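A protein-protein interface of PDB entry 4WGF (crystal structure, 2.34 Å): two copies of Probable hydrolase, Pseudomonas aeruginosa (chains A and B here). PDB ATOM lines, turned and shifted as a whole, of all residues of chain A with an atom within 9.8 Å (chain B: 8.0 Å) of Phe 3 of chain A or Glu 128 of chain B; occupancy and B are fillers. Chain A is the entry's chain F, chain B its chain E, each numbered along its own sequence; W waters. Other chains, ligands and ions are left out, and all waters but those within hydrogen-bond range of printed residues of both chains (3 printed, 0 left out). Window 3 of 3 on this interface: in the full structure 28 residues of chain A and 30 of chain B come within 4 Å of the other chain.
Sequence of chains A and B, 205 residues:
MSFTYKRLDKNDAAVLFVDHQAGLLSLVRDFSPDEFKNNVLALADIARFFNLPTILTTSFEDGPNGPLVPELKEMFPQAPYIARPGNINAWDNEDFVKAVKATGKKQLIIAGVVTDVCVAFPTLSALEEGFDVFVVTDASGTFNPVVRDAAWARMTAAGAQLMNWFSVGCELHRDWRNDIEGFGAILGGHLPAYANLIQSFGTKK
The side-chain carboxylate of Glu 128 of chain B is in hydrogen-bond range of the backbone NH of Tyr 5 of chain A, 2.7 Å away.
NH2 of Arg 154 of chain B lies within salt-bridge range of OE2 of Glu 171 of chain A.
The guanidinium group of Arg 7 of chain A lies close to the side-chain amide nitrogen of Asn 89 of chain B (3.5 Å).
The guanidinium group (NE) of Arg 154 of chain B sits at hydrogen-bond distance from the side-chain amide oxygen (OE1) of Gln 161 of chain A (2.8 Å).
No residue of chain B comes within 4 Å of Ser 2 of chain A.
Of the printed residues of chain B, Phe 3 of chain A touches Leu 124, Glu 128 and Ala 158.
Thr 4 of chain A touches just one residue of chain B: Glu 128 (3.6 Å).
Of the printed residues of chain B, Tyr 5 of chain A touches Asn 89 (3.8 Å), Phe 121 (3.3 Å), Leu 124 (3.4 Å), Ser 125 (3.3 Å), Glu 128 (2.7 Å) and Arg 154 (3.8 Å).
Of the printed residues of chain B, Lys 6 of chain A touches Arg 154.
Printed residues of chain B within 4 Å of Gln 161 of chain A: Arg 154 (2.8 Å).
Of the printed residues of chain A, Asn 89 of chain B touches Tyr 5 (3.8 Å) and Arg 7 (3.5 Å).
Of chain A, only Phe 3 (3.4 Å) and Tyr 5 (3.4 Å) come within 4 Å of Leu 124 of chain B.
Of chain A, only Tyr 5 (3.3 Å) comes within 4 Å of Ser 125 of chain B.
No residue of chain A comes within 4 Å of Ala 126 of chain B.
No residue of chain A comes within 4 Å of Leu 127 of chain B.
Val 133 of chain B touches none of the printed residues of chain A.
Printed residues of chain A within 4 Å of Arg 154 of chain B: Tyr 5, Lys 6, Gln 161 and Glu 171.
Printed residues of chain A within 4 Å of Ala 158 of chain B: Phe 3 (3.5 Å).
Position printed for both chains: 159.
Of the 15 pairs that touch across the chains among the printed residues, none has its exchanged pair printed and touching as well.
Of the 10 printed residues of chain A, 7 touch a printed residue of chain B.
Printed residues of chain A that touch a printed residue of chain B: Phe 3, Thr 4, Tyr 5, Lys 6, Arg 7, Gln 161 and Glu 171.
Of the 22 printed residues of chain B, 7 touch a printed residue of chain A.
Along chain B the printed residues that touch a printed residue of chain A span positions 89 to 158.
The side-chain amide nitrogen (ND2) of Asn 89 of chain B sits at hydrogen-bond distance from the side-chain hydroxyl (OG) of Ser 125 of chain B (3.0 Å).
The backbone carbonyl oxygen of Lys 6 of chain A sits at hydrogen-bond distance from the side-chain amide nitrogen of Gln 161 of chain A (2.9 Å).
The side-chain amide nitrogen of Asn 89 of chain B sits at hydrogen-bond distance from the backbone carbonyl oxygen of Phe 121 of chain B (3.3 Å).
The side-chain hydroxyl of Tyr 5 of chain A sits at hydrogen-bond distance from the side-chain carboxylate of Glu 171 of chain A, at 2.8 Å.
The side-chain amide oxygen (OD1) of Asn 89 of chain B sits at hydrogen-bond distance from the backbone NH (N) of Trp 91 of chain B.
The backbone carbonyl oxygen of Phe 121 of chain B sits at hydrogen-bond distance from the side-chain hydroxyl of Ser 125 of chain B.
Among the printed residues, pairs that only touch across the chains: Phe 3 of chain A with Leu 124 of chain B, Phe 3 of chain A with Glu 128 of chain B, Phe 3 of chain A with Ala 158 of chain B, Thr 4 of chain A with Glu 128 of chain B, Tyr 5 of chain A with Asn 89 of chain B, Tyr 5 of chain A with Phe 121 of chain B, Tyr 5 of chain A with Leu 124 of chain B, Tyr 5 of chain A with Ser 125 of chain B, Tyr 5 of chain A with Arg 154 of chain B, Lys 6 of chain A with Arg 154 of chain B and Glu 171 of chain A with Phe 121 of chain B.
Water W2 lies within hydrogen-bond range of the side-chain carboxylate (OE2) of Glu 128 of chain B (2.6 Å) and the backbone carbonyl oxygen (O) of Tyr 5 of chain A (3.2 Å).
Water W3 lies within hydrogen-bond range of O of Phe 3 of chain A and O of Glu 128 of chain B.
Water W1 lies within hydrogen-bond range of NH1 of Arg 7 of chain A, OH of Tyr 5 of chain A and ND2 of Asn 89 of chain B.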
ATOM      1  N   SER A   2     -17.366  -6.536  24.494  1.00  0.00           N
ATOM      2  CA  SER A   2     -17.884  -6.937  25.796  1.00  0.00           C
ATOM      3  C   SER A   2     -19.025  -7.934  25.643  1.00  0.00           C
ATOM      4  O   SER A   2     -18.804  -9.142  25.673  1.00  0.00           O
ATOM      5  CB  SER A   2     -18.347  -5.716  26.577  1.00  0.00           C
ATOM      6  OG  SER A   2     -18.796  -6.096  27.857  1.00  0.00           O
ATOM      7  N   PHE A   3     -20.248  -7.433  25.501  1.00  0.00           N
ATOM      8  CA  PHE A   3     -21.396  -8.317  25.322  1.00  0.00           C
ATOM      9  C   PHE A   3     -22.393  -7.728  24.334  1.00  0.00           C
ATOM     10  O   PHE A   3     -22.653  -6.524  24.338  1.00  0.00           O
ATOM     11  CB  PHE A   3     -22.099  -8.606  26.653  1.00  0.00           C
ATOM     12  CG  PHE A   3     -23.415  -9.317  26.491  1.00  0.00           C
ATOM     13  CD1 PHE A   3     -23.444 -10.659  26.145  1.00  0.00           C
ATOM     14  CD2 PHE A   3     -24.618  -8.652  26.676  1.00  0.00           C
ATOM     15  CE1 PHE A   3     -24.643 -11.325  25.983  1.00  0.00           C
ATOM     16  CE2 PHE A   3     -25.824  -9.316  26.517  1.00  0.00           C
ATOM     17  CZ  PHE A   3     -25.834 -10.654  26.169  1.00  0.00           C
ATOM     18  N   THR A   4     -22.952  -8.589  23.491  1.00  0.00           N
ATOM     19  CA  THR A   4     -23.962  -8.167  22.533  1.00  0.00           C
ATOM     20  C   THR A   4     -25.279  -8.893  22.772  1.00  0.00           C
ATOM     21  O   THR A   4     -25.347 -10.121  22.715  1.00  0.00           O
ATOM     22  CB  THR A   4     -23.505  -8.418  21.085  1.00  0.00           C
ATOM     23  OG1 THR A   4     -22.309  -7.674  20.821  1.00  0.00           O
ATOM     24  CG2 THR A   4     -24.584  -7.988  20.110  1.00  0.00           C
ATOM     25  N   TYR A   5     -26.323  -8.120  23.041  1.00  0.00           N
ATOM     26  CA  TYR A   5     -27.662  -8.652  23.240  1.00  0.00           C
ATOM     27  C   TYR A   5     -28.298  -9.024  21.902  1.00  0.00           C
ATOM     28  O   TYR A   5     -28.967  -8.199  21.282  1.00  0.00           O
ATOM     29  CB  TYR A   5     -28.521  -7.622  23.985  1.00  0.00           C
ATOM     30  CG  TYR A   5     -29.925  -8.059  24.357  1.00  0.00           C
ATOM     31  CD1 TYR A   5     -30.314  -9.391  24.288  1.00  0.00           C
ATOM     32  CD2 TYR A   5     -30.862  -7.127  24.786  1.00  0.00           C
ATOM     33  CE1 TYR A   5     -31.598  -9.779  24.628  1.00  0.00           C
ATOM     34  CE2 TYR A   5     -32.146  -7.506  25.131  1.00  0.00           C
ATOM     35  CZ  TYR A   5     -32.509  -8.833  25.051  1.00  0.00           C
ATOM     36  OH  TYR A   5     -33.787  -9.209  25.394  1.00  0.00           O
ATOM     37  N   LYS A   6     -28.098 -10.262  21.459  1.00  0.00           N
ATOM     38  CA  LYS A   6     -28.739 -10.730  20.235  1.00  0.00           C
ATOM     39  C   LYS A   6     -30.148 -11.214  20.524  1.00  0.00           C
ATOM     40  O   LYS A   6     -30.365 -12.391  20.815  1.00  0.00           O
ATOM     41  CB  LYS A   6     -27.931 -11.843  19.565  1.00  0.00           C
ATOM     42  CG  LYS A   6     -26.564 -11.419  19.076  1.00  0.00           C
ATOM     43  CD  LYS A   6     -25.853 -12.578  18.403  1.00  0.00           C
ATOM     44  CE  LYS A   6     -24.382 -12.277  18.188  1.00  0.00           C
ATOM     45  NZ  LYS A   6     -24.203 -11.106  17.278  1.00  0.00           N
ATOM     46  N   ARG A   7     -31.102 -10.294  20.454  1.00  0.00           N
ATOM     47  CA  ARG A   7     -32.485 -10.613  20.760  1.00  0.00           C
ATOM     48  C   ARG A   7     -33.259 -10.895  19.483  1.00  0.00           C
ATOM     49  O   ARG A   7     -32.853 -10.483  18.395  1.00  0.00           O
ATOM     50  CB  ARG A   7     -33.140  -9.480  21.555  1.00  0.00           C
ATOM     51  CG  ARG A   7     -33.027  -8.095  20.944  1.00  0.00           C
ATOM     52  CD  ARG A   7     -33.768  -7.097  21.821  1.00  0.00           C
ATOM     53  NE  ARG A   7     -33.636  -5.716  21.369  1.00  0.00           N
ATOM     54  CZ  ARG A   7     -34.214  -4.682  21.973  1.00  0.00           C
ATOM     55  NH1 ARG A   7     -34.960  -4.877  23.051  1.00  0.00           N
ATOM     56  NH2 ARG A   7     -34.047  -3.455  21.500  1.00  0.00           N
ATOM     57  N   PHE A 134     -32.249 -20.012  18.968  1.00  0.00           N
ATOM     58  CA  PHE A 134     -33.044 -19.763  20.160  1.00  0.00           C
ATOM     59  C   PHE A 134     -33.895 -20.991  20.450  1.00  0.00           C
ATOM     60  O   PHE A 134     -34.803 -21.317  19.688  1.00  0.00           O
ATOM     61  CB  PHE A 134     -33.926 -18.524  19.970  1.00  0.00           C
ATOM     62  CG  PHE A 134     -33.154 -17.266  19.675  1.00  0.00           C
ATOM     63  CD1 PHE A 134     -32.647 -17.028  18.407  1.00  0.00           C
ATOM     64  CD2 PHE A 134     -32.949 -16.314  20.660  1.00  0.00           C
ATOM     65  CE1 PHE A 134     -31.941 -15.872  18.131  1.00  0.00           C
ATOM     66  CE2 PHE A 134     -32.245 -15.155  20.390  1.00  0.00           C
ATOM     67  CZ  PHE A 134     -31.741 -14.934  19.123  1.00  0.00           C
ATOM     68  N   GLY A 159     -23.365 -22.072  22.553  1.00  0.00           N
ATOM     69  CA  GLY A 159     -23.757 -20.697  22.305  1.00  0.00           C
ATOM     70  C   GLY A 159     -25.230 -20.536  21.980  1.00  0.00           C
ATOM     71  O   GLY A 159     -25.660 -19.476  21.527  1.00  0.00           O
ATOM     72  N   GLN A 161     -29.122 -19.937  22.772  1.00  0.00           N
ATOM     73  CA  GLN A 161     -29.846 -19.167  23.775  1.00  0.00           C
ATOM     74  C   GLN A 161     -31.091 -19.917  24.233  1.00  0.00           C
ATOM     75  O   GLN A 161     -32.000 -20.174  23.444  1.00  0.00           O
ATOM     76  CB  GLN A 161     -30.218 -17.786  23.231  1.00  0.00           C
ATOM     77  CG  GLN A 161     -29.013 -16.922  22.890  1.00  0.00           C
ATOM     78  CD  GLN A 161     -29.366 -15.457  22.741  1.00  0.00           C
ATOM     79  OE1 GLN A 161     -29.977 -14.861  23.629  1.00  0.00           O
ATOM     80  NE2 GLN A 161     -28.983 -14.865  21.614  1.00  0.00           N
ATOM     81  N   GLU A 171     -40.131 -11.014  23.236  1.00  0.00           N
ATOM     82  CA  GLU A 171     -38.942 -10.477  22.587  1.00  0.00           C
ATOM     83  C   GLU A 171     -39.220 -10.150  21.124  1.00  0.00           C
ATOM     84  O   GLU A 171     -38.618  -9.241  20.555  1.00  0.00           O
ATOM     85  CB  GLU A 171     -37.774 -11.458  22.708  1.00  0.00           C
ATOM     86  CG  GLU A 171     -36.424 -10.852  22.366  1.00  0.00           C
ATOM     87  CD  GLU A 171     -35.267 -11.620  22.976  1.00  0.00           C
ATOM     88  OE1 GLU A 171     -34.952 -11.382  24.161  1.00  0.00           O
ATOM     89  OE2 GLU A 171     -34.669 -12.459  22.270  1.00  0.00           O
ATOM     90  N   ASN B  89     -39.549  -4.730  27.295  1.00  0.00           N
ATOM     91  CA  ASN B  89     -38.211  -4.507  27.827  1.00  0.00           C
ATOM     92  C   ASN B  89     -38.125  -3.078  28.349  1.00  0.00           C
ATOM     93  O   ASN B  89     -38.262  -2.123  27.585  1.00  0.00           O
ATOM     94  CB  ASN B  89     -37.143  -4.762  26.757  1.00  0.00           C
ATOM     95  CG  ASN B  89     -35.721  -4.679  27.302  1.00  0.00           C
ATOM     96  OD1 ASN B  89     -35.482  -4.170  28.397  1.00  0.00           O
ATOM     97  ND2 ASN B  89     -34.768  -5.183  26.529  1.00  0.00           N
ATOM     98  N   TRP B  91     -35.729  -1.367  29.161  1.00  0.00           N
ATOM     99  CA  TRP B  91     -34.601  -0.627  28.611  1.00  0.00           C
ATOM    100  C   TRP B  91     -34.952   0.018  27.272  1.00  0.00           C
ATOM    101  O   TRP B  91     -34.216   0.869  26.773  1.00  0.00           O
ATOM    102  CB  TRP B  91     -33.389  -1.544  28.456  1.00  0.00           C
ATOM    103  CG  TRP B  91     -32.080  -0.827  28.585  1.00  0.00           C
ATOM    104  CD1 TRP B  91     -31.317  -0.321  27.574  1.00  0.00           C
ATOM    105  CD2 TRP B  91     -31.386  -0.529  29.802  1.00  0.00           C
ATOM    106  NE1 TRP B  91     -30.187   0.269  28.086  1.00  0.00           N
ATOM    107  CE2 TRP B  91     -30.206   0.156  29.452  1.00  0.00           C
ATOM    108  CE3 TRP B  91     -31.646  -0.777  31.153  1.00  0.00           C
ATOM    109  CZ2 TRP B  91     -29.287   0.596  30.403  1.00  0.00           C
ATOM    110  CZ3 TRP B  91     -30.734  -0.340  32.095  1.00  0.00           C
ATOM    111  CH2 TRP B  91     -29.570   0.339  31.717  1.00  0.00           C
ATOM    112  N   ALA B 120     -34.980 -10.466  32.631  1.00  0.00           N
ATOM    113  CA  ALA B 120     -33.933 -10.905  31.717  1.00  0.00           C
ATOM    114  C   ALA B 120     -33.615  -9.865  30.648  1.00  0.00           C
ATOM    115  O   ALA B 120     -32.450  -9.561  30.405  1.00  0.00           O
ATOM    116  CB  ALA B 120     -34.328 -12.221  31.065  1.00  0.00           C
ATOM    117  N   PHE B 121     -34.650  -9.313  30.020  1.00  0.00           N
ATOM    118  CA  PHE B 121     -34.456  -8.401  28.893  1.00  0.00           C
ATOM    119  C   PHE B 121     -33.685  -7.131  29.280  1.00  0.00           C
ATOM    120  O   PHE B 121     -32.714  -6.784  28.607  1.00  0.00           O
ATOM    121  CB  PHE B 121     -35.800  -8.018  28.250  1.00  0.00           C
ATOM    122  CG  PHE B 121     -36.506  -9.159  27.559  1.00  0.00           C
ATOM    123  CD1 PHE B 121     -35.957 -10.432  27.528  1.00  0.00           C
ATOM    124  CD2 PHE B 121     -37.722  -8.947  26.929  1.00  0.00           C
ATOM    125  CE1 PHE B 121     -36.613 -11.471  26.892  1.00  0.00           C
ATOM    126  CE2 PHE B 121     -38.381  -9.981  26.290  1.00  0.00           C
ATOM    127  CZ  PHE B 121     -37.826 -11.244  26.271  1.00  0.00           C
ATOM    128  N   PRO B 122     -34.102  -6.427  30.353  1.00  0.00           N
ATOM    129  CA  PRO B 122     -33.298  -5.245  30.688  1.00  0.00           C
ATOM    130  C   PRO B 122     -31.928  -5.599  31.265  1.00  0.00           C
ATOM    131  O   PRO B 122     -31.006  -4.791  31.171  1.00  0.00           O
ATOM    132  CB  PRO B 122     -34.153  -4.521  31.732  1.00  0.00           C
ATOM    133  CG  PRO B 122     -34.970  -5.589  32.347  1.00  0.00           C
ATOM    134  CD  PRO B 122     -35.272  -6.556  31.243  1.00  0.00           C
ATOM    135  N   THR B 123     -31.801  -6.786  31.851  1.00  0.00           N
ATOM    136  CA  THR B 123     -30.512  -7.261  32.344  1.00  0.00           C
ATOM    137  C   THR B 123     -29.527  -7.413  31.192  1.00  0.00           C
ATOM    138  O   THR B 123     -28.396  -6.934  31.257  1.00  0.00           O
ATOM    139  CB  THR B 123     -30.646  -8.604  33.087  1.00  0.00           C
ATOM    140  OG1 THR B 123     -31.350  -8.400  34.318  1.00  0.00           O
ATOM    141  CG2 THR B 123     -29.276  -9.196  33.385  1.00  0.00           C
ATOM    142  N   LEU B 124     -29.974  -8.079  30.132  1.00  0.00           N
ATOM    143  CA  LEU B 124     -29.149  -8.287  28.950  1.00  0.00           C
ATOM    144  C   LEU B 124     -28.831  -6.955  28.274  1.00  0.00           C
ATOM    145  O   LEU B 124     -27.721  -6.744  27.784  1.00  0.00           O
ATOM    146  CB  LEU B 124     -29.849  -9.233  27.971  1.00  0.00           C
ATOM    147  CG  LEU B 124     -30.197 -10.614  28.536  1.00  0.00           C
ATOM    148  CD1 LEU B 124     -31.062 -11.418  27.578  1.00  0.00           C
ATOM    149  CD2 LEU B 124     -28.945 -11.382  28.894  1.00  0.00           C
ATOM    150  N   SER B 125     -29.813  -6.061  28.252  1.00  0.00           N
ATOM    151  CA  SER B 125     -29.636  -4.743  27.654  1.00  0.00           C
ATOM    152  C   SER B 125     -28.627  -3.906  28.437  1.00  0.00           C
ATOM    153  O   SER B 125     -27.793  -3.218  27.851  1.00  0.00           O
ATOM    154  CB  SER B 125     -30.975  -4.007  27.577  1.00  0.00           C
ATOM    155  OG  SER B 125     -31.862  -4.643  26.674  1.00  0.00           O
ATOM    156  N   ALA B 126     -28.715  -3.964  29.763  1.00  0.00           N
ATOM    157  CA  ALA B 126     -27.822  -3.200  30.629  1.00  0.00           C
ATOM    158  C   ALA B 126     -26.396  -3.744  30.591  1.00  0.00           C
ATOM    159  O   ALA B 126     -25.430  -2.980  30.625  1.00  0.00           O
ATOM    160  CB  ALA B 126     -28.349  -3.192  32.056  1.00  0.00           C
ATOM    161  N   LEU B 127     -26.272  -5.066  30.525  1.00  0.00           N
ATOM    162  CA  LEU B 127     -24.969  -5.713  30.420  1.00  0.00           C
ATOM    163  C   LEU B 127     -24.294  -5.314  29.116  1.00  0.00           C
ATOM    164  O   LEU B 127     -23.072  -5.183  29.046  1.00  0.00           O
ATOM    165  CB  LEU B 127     -25.104  -7.234  30.506  1.00  0.00           C
ATOM    166  CG  LEU B 127     -25.367  -7.813  31.897  1.00  0.00           C
ATOM    167  CD1 LEU B 127     -25.738  -9.281  31.805  1.00  0.00           C
ATOM    168  CD2 LEU B 127     -24.155  -7.624  32.795  1.00  0.00           C
ATOM    169  N   GLU B 128     -25.109  -5.129  28.084  1.00  0.00           N
ATOM    170  CA  GLU B 128     -24.625  -4.712  26.778  1.00  0.00           C
ATOM    171  C   GLU B 128     -24.031  -3.307  26.849  1.00  0.00           C
ATOM    172  O   GLU B 128     -23.094  -2.981  26.120  1.00  0.00           O
ATOM    173  CB  GLU B 128     -25.763  -4.770  25.755  1.00  0.00           C
ATOM    174  CG  GLU B 128     -25.350  -4.519  24.317  1.00  0.00           C
ATOM    175  CD  GLU B 128     -26.506  -4.683  23.346  1.00  0.00           C
ATOM    176  OE1 GLU B 128     -27.532  -3.990  23.516  1.00  0.00           O
ATOM    177  OE2 GLU B 128     -26.389  -5.504  22.412  1.00  0.00           O
ATOM    178  N   GLU B 129     -24.583  -2.477  27.728  1.00  0.00           N
ATOM    179  CA  GLU B 129     -24.108  -1.105  27.896  1.00  0.00           C
ATOM    180  C   GLU B 129     -22.991  -0.973  28.931  1.00  0.00           C
ATOM    181  O   GLU B 129     -22.569   0.138  29.247  1.00  0.00           O
ATOM    182  CB  GLU B 129     -25.267  -0.183  28.278  1.00  0.00           C
ATOM    183  CG  GLU B 129     -26.265   0.057  27.158  1.00  0.00           C
ATOM    184  CD  GLU B 129     -26.973   1.391  27.288  1.00  0.00           C
ATOM    185  OE1 GLU B 129     -26.400   2.313  27.907  1.00  0.00           O
ATOM    186  OE2 GLU B 129     -28.102   1.520  26.771  1.00  0.00           O
ATOM    187  N   GLY B 130     -22.510  -2.095  29.453  1.00  0.00           N
ATOM    188  CA  GLY B 130     -21.364  -2.081  30.346  1.00  0.00           C
ATOM    189  C   GLY B 130     -21.666  -2.007  31.828  1.00  0.00           C
ATOM    190  O   GLY B 130     -20.757  -1.850  32.642  1.00  0.00           O
ATOM    191  N   PHE B 131     -22.938  -2.141  32.183  1.00  0.00           N
ATOM    192  CA  PHE B 131     -23.337  -2.152  33.584  1.00  0.00           C
ATOM    193  C   PHE B 131     -23.015  -3.476  34.269  1.00  0.00           C
ATOM    194  O   PHE B 131     -23.018  -4.534  33.637  1.00  0.00           O
ATOM    195  CB  PHE B 131     -24.833  -1.862  33.717  1.00  0.00           C
ATOM    196  CG  PHE B 131     -25.196  -0.419  33.507  1.00  0.00           C
ATOM    197  CD1 PHE B 131     -25.200   0.466  34.571  1.00  0.00           C
ATOM    198  CD2 PHE B 131     -25.545   0.050  32.251  1.00  0.00           C
ATOM    199  CE1 PHE B 131     -25.538   1.794  34.388  1.00  0.00           C
ATOM    200  CE2 PHE B 131     -25.883   1.377  32.061  1.00  0.00           C
ATOM    201  CZ  PHE B 131     -25.879   2.249  33.133  1.00  0.00           C
ATOM    202  N   VAL B 133     -24.626  -6.011  36.499  1.00  0.00           N
ATOM    203  CA  VAL B 133     -25.994  -6.328  36.879  1.00  0.00           C
ATOM    204  C   VAL B 133     -26.037  -7.472  37.883  1.00  0.00           C
ATOM    205  O   VAL B 133     -25.493  -8.551  37.644  1.00  0.00           O
ATOM    206  CB  VAL B 133     -26.850  -6.688  35.652  1.00  0.00           C
ATOM    207  CG1 VAL B 133     -28.292  -6.924  36.067  1.00  0.00           C
ATOM    208  CG2 VAL B 133     -26.771  -5.579  34.612  1.00  0.00           C
ATOM    209  N   ARG B 154     -29.448 -17.938  30.407  1.00  0.00           N
ATOM    210  CA  ARG B 154     -29.307 -16.868  29.430  1.00  0.00           C
ATOM    211  C   ARG B 154     -28.625 -15.648  30.039  1.00  0.00           C
ATOM    212  O   ARG B 154     -27.837 -14.971  29.377  1.00  0.00           O
ATOM    213  CB  ARG B 154     -30.667 -16.474  28.858  1.00  0.00           C
ATOM    214  CG  ARG B 154     -30.571 -15.714  27.547  1.00  0.00           C
ATOM    215  CD  ARG B 154     -31.926 -15.221  27.073  1.00  0.00           C
ATOM    216  NE  ARG B 154     -31.842 -14.634  25.739  1.00  0.00           N
ATOM    217  CZ  ARG B 154     -32.759 -13.824  25.217  1.00  0.00           C
ATOM    218  NH1 ARG B 154     -33.833 -13.493  25.919  1.00  0.00           N
ATOM    219  NH2 ARG B 154     -32.594 -13.339  23.993  1.00  0.00           N
ATOM    220  N   MET B 155     -28.932 -15.367  31.301  1.00  0.00           N
ATOM    221  CA  MET B 155     -28.348 -14.222  31.989  1.00  0.00           C
ATOM    222  C   MET B 155     -26.918 -14.510  32.434  1.00  0.00           C
ATOM    223  O   MET B 155     -26.064 -13.624  32.408  1.00  0.00           O
ATOM    224  CB  MET B 155     -29.209 -13.824  33.191  1.00  0.00           C
ATOM    225  CG  MET B 155     -30.555 -13.224  32.810  1.00  0.00           C
ATOM    226  SD  MET B 155     -31.582 -12.595  34.346  1.00  0.00           S
ATOM    227  CE  MET B 155     -31.887 -14.306  35.234  1.00  0.00           C
ATOM    228  N   THR B 156     -26.666 -15.752  32.838  1.00  0.00           N
ATOM    229  CA  THR B 156     -25.329 -16.182  33.243  1.00  0.00           C
ATOM    230  C   THR B 156     -24.347 -16.052  32.084  1.00  0.00           C
ATOM    231  O   THR B 156     -23.237 -15.543  32.250  1.00  0.00           O
ATOM    232  CB  THR B 156     -25.332 -17.641  33.752  1.00  0.00           C
ATOM    233  OG1 THR B 156     -25.778 -17.673  35.112  1.00  0.00           O
ATOM    234  CG2 THR B 156     -23.941 -18.252  33.669  1.00  0.00           C
ATOM    235  N   ALA B 157     -24.773 -16.501  30.908  1.00  0.00           N
ATOM    236  CA  ALA B 157     -23.936 -16.468  29.713  1.00  0.00           C
ATOM    237  C   ALA B 157     -23.596 -15.035  29.315  1.00  0.00           C
ATOM    238  O   ALA B 157     -22.621 -14.793  28.605  1.00  0.00           O
ATOM    239  CB  ALA B 157     -24.626 -17.186  28.564  1.00  0.00           C
ATOM    240  N   ALA B 158     -24.409 -14.091  29.776  1.00  0.00           N
ATOM    241  CA  ALA B 158     -24.209 -12.685  29.454  1.00  0.00           C
ATOM    242  C   ALA B 158     -23.324 -11.988  30.480  1.00  0.00           C
ATOM    243  O   ALA B 158     -22.864 -10.870  30.253  1.00  0.00           O
ATOM    244  CB  ALA B 158     -25.538 -11.981  29.356  1.00  0.00           C
ATOM    245  N   GLY B 159     -23.093 -12.647  31.611  1.00  0.00           N
ATOM    246  CA  GLY B 159     -22.214 -12.101  32.630  1.00  0.00           C
ATOM    247  C   GLY B 159     -22.942 -11.520  33.827  1.00  0.00           C
ATOM    248  O   GLY B 159     -22.345 -10.819  34.642  1.00  0.00           O
ATOM    249  N   ALA B 160     -24.236 -11.802  33.933  1.00  0.00           N
ATOM    250  CA  ALA B 160     -25.017 -11.337  35.073  1.00  0.00           C
ATOM    251  C   ALA B 160     -24.643 -12.115  36.328  1.00  0.00           C
ATOM    252  O   ALA B 160     -24.340 -13.306  36.261  1.00  0.00           O
ATOM    253  CB  ALA B 160     -26.504 -11.466  34.790  1.00  0.00           C
HETATM  254  O   HOH W   1     -35.838  -7.249  24.491  1.00  0.00           O
HETATM  255  O   HOH W   2     -27.756  -5.434  20.252  1.00  0.00           O
HETATM  256  O   HOH W   3     -21.189  -4.416  24.523  1.00  0.00           O
